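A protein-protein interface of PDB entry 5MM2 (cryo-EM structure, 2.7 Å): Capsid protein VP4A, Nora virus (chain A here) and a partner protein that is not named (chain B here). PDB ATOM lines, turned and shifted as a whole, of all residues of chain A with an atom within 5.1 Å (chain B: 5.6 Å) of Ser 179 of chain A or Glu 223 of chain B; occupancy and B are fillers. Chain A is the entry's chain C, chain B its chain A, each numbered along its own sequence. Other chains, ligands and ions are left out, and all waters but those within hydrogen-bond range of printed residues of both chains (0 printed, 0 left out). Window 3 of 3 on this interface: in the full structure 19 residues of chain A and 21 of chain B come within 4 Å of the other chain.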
ATOM      1  N   ILE A  70      -5.222  34.603  11.077  1.00  0.00           N
ATOM      2  CA  ILE A  70      -3.939  34.682  10.375  1.00  0.00           C
ATOM      3  C   ILE A  70      -4.137  34.714   8.865  1.00  0.00           C
ATOM      4  O   ILE A  70      -4.852  33.880   8.308  1.00  0.00           O
ATOM      5  CB  ILE A  70      -3.069  33.477  10.771  1.00  0.00           C
ATOM      6  CG1 ILE A  70      -2.838  33.441  12.278  1.00  0.00           C
ATOM      7  CG2 ILE A  70      -1.743  33.493  10.038  1.00  0.00           C
ATOM      8  CD1 ILE A  70      -2.200  32.161  12.750  1.00  0.00           C
ATOM      9  N   PRO A  72      -1.761  34.577   5.568  1.00  0.00           N
ATOM     10  CA  PRO A  72      -0.387  34.449   5.070  1.00  0.00           C
ATOM     11  C   PRO A  72      -0.175  35.279   3.814  1.00  0.00           C
ATOM     12  O   PRO A  72      -0.991  35.253   2.894  1.00  0.00           O
ATOM     13  CB  PRO A  72      -0.260  32.952   4.782  1.00  0.00           C
ATOM     14  CG  PRO A  72      -1.309  32.331   5.595  1.00  0.00           C
ATOM     15  CD  PRO A  72      -2.446  33.281   5.579  1.00  0.00           C
ATOM     16  N   TRP A 174     -14.790  32.753  10.427  1.00  0.00           N
ATOM     17  CA  TRP A 174     -14.068  31.796   9.594  1.00  0.00           C
ATOM     18  C   TRP A 174     -13.302  30.829  10.482  1.00  0.00           C
ATOM     19  O   TRP A 174     -12.395  31.232  11.210  1.00  0.00           O
ATOM     20  CB  TRP A 174     -13.117  32.527   8.654  1.00  0.00           C
ATOM     21  CG  TRP A 174     -12.310  31.634   7.755  1.00  0.00           C
ATOM     22  CD1 TRP A 174     -11.024  31.237   7.942  1.00  0.00           C
ATOM     23  CD2 TRP A 174     -12.723  31.063   6.516  1.00  0.00           C
ATOM     24  NE1 TRP A 174     -10.619  30.445   6.910  1.00  0.00           N
ATOM     25  CE2 TRP A 174     -11.645  30.324   6.018  1.00  0.00           C
ATOM     26  CE3 TRP A 174     -13.904  31.103   5.780  1.00  0.00           C
ATOM     27  CZ2 TRP A 174     -11.710  29.630   4.827  1.00  0.00           C
ATOM     28  CZ3 TRP A 174     -13.963  30.414   4.599  1.00  0.00           C
ATOM     29  CH2 TRP A 174     -12.877  29.686   4.135  1.00  0.00           C
ATOM     30  N   ASN A 176     -11.303  27.199  10.005  1.00  0.00           N
ATOM     31  CA  ASN A 176     -10.853  26.185   9.073  1.00  0.00           C
ATOM     32  C   ASN A 176      -9.410  25.843   9.401  1.00  0.00           C
ATOM     33  O   ASN A 176      -8.673  26.683   9.918  1.00  0.00           O
ATOM     34  CB  ASN A 176     -10.969  26.678   7.636  1.00  0.00           C
ATOM     35  CG  ASN A 176     -10.887  25.569   6.650  1.00  0.00           C
ATOM     36  OD1 ASN A 176     -10.812  24.405   7.016  1.00  0.00           O
ATOM     37  ND2 ASN A 176     -10.900  25.914   5.388  1.00  0.00           N
ATOM     38  N   ASP A 177      -9.004  24.611   9.084  1.00  0.00           N
ATOM     39  CA  ASP A 177      -7.631  24.204   9.362  1.00  0.00           C
ATOM     40  C   ASP A 177      -6.643  24.739   8.344  1.00  0.00           C
ATOM     41  O   ASP A 177      -5.434  24.628   8.548  1.00  0.00           O
ATOM     42  CB  ASP A 177      -7.514  22.684   9.442  1.00  0.00           C
ATOM     43  CG  ASP A 177      -7.972  21.989   8.195  1.00  0.00           C
ATOM     44  OD1 ASP A 177      -8.577  22.630   7.321  1.00  0.00           O
ATOM     45  OD2 ASP A 177      -7.702  20.777   8.073  1.00  0.00           O
ATOM     46  N   LEU A 178      -7.139  25.289   7.251  1.00  0.00           N
ATOM     47  CA  LEU A 178      -6.355  26.019   6.273  1.00  0.00           C
ATOM     48  C   LEU A 178      -6.926  27.415   6.160  1.00  0.00           C
ATOM     49  O   LEU A 178      -8.116  27.579   5.883  1.00  0.00           O
ATOM     50  CB  LEU A 178      -6.381  25.322   4.915  1.00  0.00           C
ATOM     51  CG  LEU A 178      -5.204  24.444   4.522  1.00  0.00           C
ATOM     52  CD1 LEU A 178      -4.903  23.387   5.525  1.00  0.00           C
ATOM     53  CD2 LEU A 178      -5.528  23.817   3.202  1.00  0.00           C
ATOM     54  N   SER A 179      -6.093  28.415   6.397  1.00  0.00           N
ATOM     55  CA  SER A 179      -6.433  29.757   5.972  1.00  0.00           C
ATOM     56  C   SER A 179      -6.387  29.808   4.455  1.00  0.00           C
ATOM     57  O   SER A 179      -5.660  29.042   3.826  1.00  0.00           O
ATOM     58  CB  SER A 179      -5.448  30.755   6.558  1.00  0.00           C
ATOM     59  OG  SER A 179      -5.470  30.688   7.966  1.00  0.00           O
ATOM     60  N   THR A 180      -7.188  30.701   3.874  1.00  0.00           N
ATOM     61  CA  THR A 180      -7.207  31.003   2.440  1.00  0.00           C
ATOM     62  C   THR A 180      -7.419  29.745   1.588  1.00  0.00           C
ATOM     63  O   THR A 180      -6.493  29.200   1.000  1.00  0.00           O
ATOM     64  CB  THR A 180      -5.949  31.764   1.992  1.00  0.00           C
ATOM     65  OG1 THR A 180      -4.795  30.931   2.105  1.00  0.00           O
ATOM     66  CG2 THR A 180      -5.745  32.994   2.835  1.00  0.00           C
ATOM     67  N   VAL A 181      -8.658  29.258   1.591  1.00  0.00           N
ATOM     68  CA  VAL A 181      -9.011  28.233   0.622  1.00  0.00           C
ATOM     69  C   VAL A 181      -9.087  28.834  -0.773  1.00  0.00           C
ATOM     70  O   VAL A 181      -9.236  30.041  -0.954  1.00  0.00           O
ATOM     71  CB  VAL A 181     -10.334  27.551   0.982  1.00  0.00           C
ATOM     72  CG1 VAL A 181     -10.198  26.849   2.275  1.00  0.00           C
ATOM     73  CG2 VAL A 181     -11.436  28.567   1.043  1.00  0.00           C
ATOM     74  N   ASN B  29       1.968  29.581  11.367  1.00  0.00           N
ATOM     75  CA  ASN B  29       0.792  28.908  10.807  1.00  0.00           C
ATOM     76  C   ASN B  29      -0.058  28.196  11.838  1.00  0.00           C
ATOM     77  O   ASN B  29      -1.171  27.799  11.515  1.00  0.00           O
ATOM     78  CB  ASN B  29       1.108  27.873   9.717  1.00  0.00           C
ATOM     79  CG  ASN B  29       1.601  28.484   8.450  1.00  0.00           C
ATOM     80  OD1 ASN B  29       2.752  28.294   8.071  1.00  0.00           O
ATOM     81  ND2 ASN B  29       0.728  29.189   7.755  1.00  0.00           N
ATOM     82  N   VAL B  30       0.402  28.041  13.057  1.00  0.00           N
ATOM     83  CA  VAL B  30      -0.386  27.355  14.067  1.00  0.00           C
ATOM     84  C   VAL B  30      -1.074  28.409  14.916  1.00  0.00           C
ATOM     85  O   VAL B  30      -0.511  29.473  15.197  1.00  0.00           O
ATOM     86  CB  VAL B  30       0.476  26.371  14.888  1.00  0.00           C
ATOM     87  CG1 VAL B  30       1.559  27.066  15.669  1.00  0.00           C
ATOM     88  CG2 VAL B  30      -0.382  25.521  15.796  1.00  0.00           C
ATOM     89  N   HIS B  31      -2.338  28.165  15.234  1.00  0.00           N
ATOM     90  CA  HIS B  31      -3.187  29.179  15.839  1.00  0.00           C
ATOM     91  C   HIS B  31      -3.339  28.817  17.309  1.00  0.00           C
ATOM     92  O   HIS B  31      -4.308  28.203  17.731  1.00  0.00           O
ATOM     93  CB  HIS B  31      -4.512  29.241  15.105  1.00  0.00           C
ATOM     94  CG  HIS B  31      -5.277  30.501  15.323  1.00  0.00           C
ATOM     95  ND1 HIS B  31      -6.547  30.685  14.832  1.00  0.00           N
ATOM     96  CD2 HIS B  31      -4.958  31.639  15.977  1.00  0.00           C
ATOM     97  CE1 HIS B  31      -6.977  31.886  15.166  1.00  0.00           C
ATOM     98  NE2 HIS B  31      -6.033  32.483  15.866  1.00  0.00           N
ATOM     99  N   LEU B  34      -6.420  29.707  20.438  1.00  0.00           N
ATOM    100  CA  LEU B  34      -7.686  29.401  19.794  1.00  0.00           C
ATOM    101  C   LEU B  34      -8.575  28.465  20.592  1.00  0.00           C
ATOM    102  O   LEU B  34      -9.795  28.636  20.586  1.00  0.00           O
ATOM    103  CB  LEU B  34      -7.407  28.806  18.428  1.00  0.00           C
ATOM    104  CG  LEU B  34      -8.558  28.543  17.478  1.00  0.00           C
ATOM    105  CD1 LEU B  34      -9.214  29.848  17.132  1.00  0.00           C
ATOM    106  CD2 LEU B  34      -8.013  27.878  16.249  1.00  0.00           C
ATOM    107  N   ILE B  92      -5.438  21.568  18.902  1.00  0.00           N
ATOM    108  CA  ILE B  92      -4.530  22.685  18.685  1.00  0.00           C
ATOM    109  C   ILE B  92      -3.259  22.413  19.475  1.00  0.00           C
ATOM    110  O   ILE B  92      -3.322  22.267  20.694  1.00  0.00           O
ATOM    111  CB  ILE B  92      -5.134  24.035  19.101  1.00  0.00           C
ATOM    112  CG1 ILE B  92      -6.374  24.389  18.290  1.00  0.00           C
ATOM    113  CG2 ILE B  92      -4.128  25.119  18.912  1.00  0.00           C
ATOM    114  CD1 ILE B  92      -7.671  24.047  18.944  1.00  0.00           C
ATOM    115  N   PRO B  93      -2.094  22.337  18.837  1.00  0.00           N
ATOM    116  CA  PRO B  93      -0.849  22.132  19.586  1.00  0.00           C
ATOM    117  C   PRO B  93      -0.493  23.326  20.456  1.00  0.00           C
ATOM    118  O   PRO B  93      -0.711  24.476  20.075  1.00  0.00           O
ATOM    119  CB  PRO B  93       0.187  21.925  18.480  1.00  0.00           C
ATOM    120  CG  PRO B  93      -0.594  21.472  17.321  1.00  0.00           C
ATOM    121  CD  PRO B  93      -1.894  22.180  17.391  1.00  0.00           C
ATOM    122  N   PHE B 221       2.166  23.539   8.040  1.00  0.00           N
ATOM    123  CA  PHE B 221       1.265  24.384   7.284  1.00  0.00           C
ATOM    124  C   PHE B 221      -0.154  24.417   7.819  1.00  0.00           C
ATOM    125  O   PHE B 221      -0.877  25.366   7.513  1.00  0.00           O
ATOM    126  CB  PHE B 221       1.235  23.972   5.801  1.00  0.00           C
ATOM    127  CG  PHE B 221       0.551  22.668   5.528  1.00  0.00           C
ATOM    128  CD1 PHE B 221       1.228  21.475   5.650  1.00  0.00           C
ATOM    129  CD2 PHE B 221      -0.752  22.644   5.066  1.00  0.00           C
ATOM    130  CE1 PHE B 221       0.596  20.284   5.381  1.00  0.00           C
ATOM    131  CE2 PHE B 221      -1.382  21.464   4.800  1.00  0.00           C
ATOM    132  CZ  PHE B 221      -0.712  20.283   4.954  1.00  0.00           C
ATOM    133  N   VAL B 222      -0.578  23.431   8.587  1.00  0.00           N
ATOM    134  CA  VAL B 222      -1.956  23.399   9.057  1.00  0.00           C
ATOM    135  C   VAL B 222      -2.125  24.373  10.207  1.00  0.00           C
ATOM    136  O   VAL B 222      -1.177  24.715  10.916  1.00  0.00           O
ATOM    137  CB  VAL B 222      -2.389  21.981   9.464  1.00  0.00           C
ATOM    138  CG1 VAL B 222      -2.344  21.068   8.277  1.00  0.00           C
ATOM    139  CG2 VAL B 222      -1.522  21.456  10.584  1.00  0.00           C
ATOM    140  N   GLU B 223      -3.355  24.827  10.383  1.00  0.00           N
ATOM    141  CA  GLU B 223      -3.679  25.790  11.419  1.00  0.00           C
ATOM    142  C   GLU B 223      -4.127  25.115  12.700  1.00  0.00           C
ATOM    143  O   GLU B 223      -3.835  25.606  13.792  1.00  0.00           O
ATOM    144  CB  GLU B 223      -4.748  26.748  10.897  1.00  0.00           C
ATOM    145  CG  GLU B 223      -5.108  27.862  11.814  1.00  0.00           C
ATOM    146  CD  GLU B 223      -6.065  28.837  11.187  1.00  0.00           C
ATOM    147  OE1 GLU B 223      -6.452  28.618  10.026  1.00  0.00           O
ATOM    148  OE2 GLU B 223      -6.429  29.826  11.852  1.00  0.00           O
ATOM    149  N   MET B 224      -4.791  23.976  12.573  1.00  0.00           N
ATOM    150  CA  MET B 224      -5.253  23.134  13.663  1.00  0.00           C
ATOM    151  C   MET B 224      -5.193  21.705  13.146  1.00  0.00           C
ATOM    152  O   MET B 224      -4.563  21.436  12.121  1.00  0.00           O
ATOM    153  CB  MET B 224      -6.652  23.579  14.109  1.00  0.00           C
ATOM    154  CG  MET B 224      -7.644  23.475  12.995  1.00  0.00           C
ATOM    155  SD  MET B 224      -9.223  24.252  13.277  1.00  0.00           S
ATOM    156  CE  MET B 224      -8.774  25.972  13.157  1.00  0.00           C
ATOM    157  N   LEU B 225      -5.856  20.783  13.823  1.00  0.00           N
ATOM    158  CA  LEU B 225      -5.682  19.378  13.495  1.00  0.00           C
ATOM    159  C   LEU B 225      -7.036  18.730  13.241  1.00  0.00           C
ATOM    160  O   LEU B 225      -7.450  17.794  13.919  1.00  0.00           O
ATOM    161  CB  LEU B 225      -4.878  18.707  14.596  1.00  0.00           C
ATOM    162  CG  LEU B 225      -3.928  17.565  14.279  1.00  0.00           C
ATOM    163  CD1 LEU B 225      -2.894  17.527  15.367  1.00  0.00           C
ATOM    164  CD2 LEU B 225      -4.620  16.255  14.192  1.00  0.00           C
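The side-chain carboxylate (OE1) of Glu 223 of chain B lies close to the backbone carbonyl oxygen (O) of Asn 176 of chain A (2.9 Å). O of Asp 177 of chain A is in hydrogen-bond range of N of Glu 223 of chain B, at 2.8 Å. The side-chain carboxylate (OE1) of Glu 223 of chain B is in hydrogen-bond range of the side-chain hydroxyl (OG) of Ser 179 of chain A (3.1 Å).
The backbone carbonyl oxygen (O) of Leu 178 of chain A sits at hydrogen-bond distance from the side-chain amide nitrogen (ND2) of Asn 176 of chain A (3.3 Å). ND1 of His 31 of chain B is in hydrogen-bond range of OE2 of Glu 223 of chain B. OD1 of Asn 176 of chain A lies close to OD1 of Asp 177 of chain A (2.9 Å). O of Ile 70 of chain A lies within hydrogen-bond range of OG of Ser 179 of chain A, at 3.3 Å.
Among the printed residues, pairs that only touch across the chains: Asn 176 of chain A with Met 224 of chain B, Asp 177 of chain A with Val 222 of chain B and Asp 177 of chain A with Met 224 of chain B.
Printed residues of chain B within 4 Å of Asn 176 of chain A: Glu 223 (2.9 Å) and Met 224 (3.3 Å). Printed residues of chain B within 4 Å of Asp 177 of chain A: Val 222 (3.7 Å), Glu 223 (2.8 Å) and Met 224 (3.6 Å). Ser 179 of chain A touches just one residue of chain B: Glu 223. Printed residues of chain A within 4 Å of Val 222 of chain B: Asp 177. Glu 223 of chain B touches three residues of chain A. Of the printed residues of chain A, Met 224 of chain B touches Asn 176 (3.3 Å) and Asp 177 (3.6 Å).
Of the 9 printed residues of chain A, 3 touch a printed residue of chain B. Among the printed residues, 6 pairs touch across the chains.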
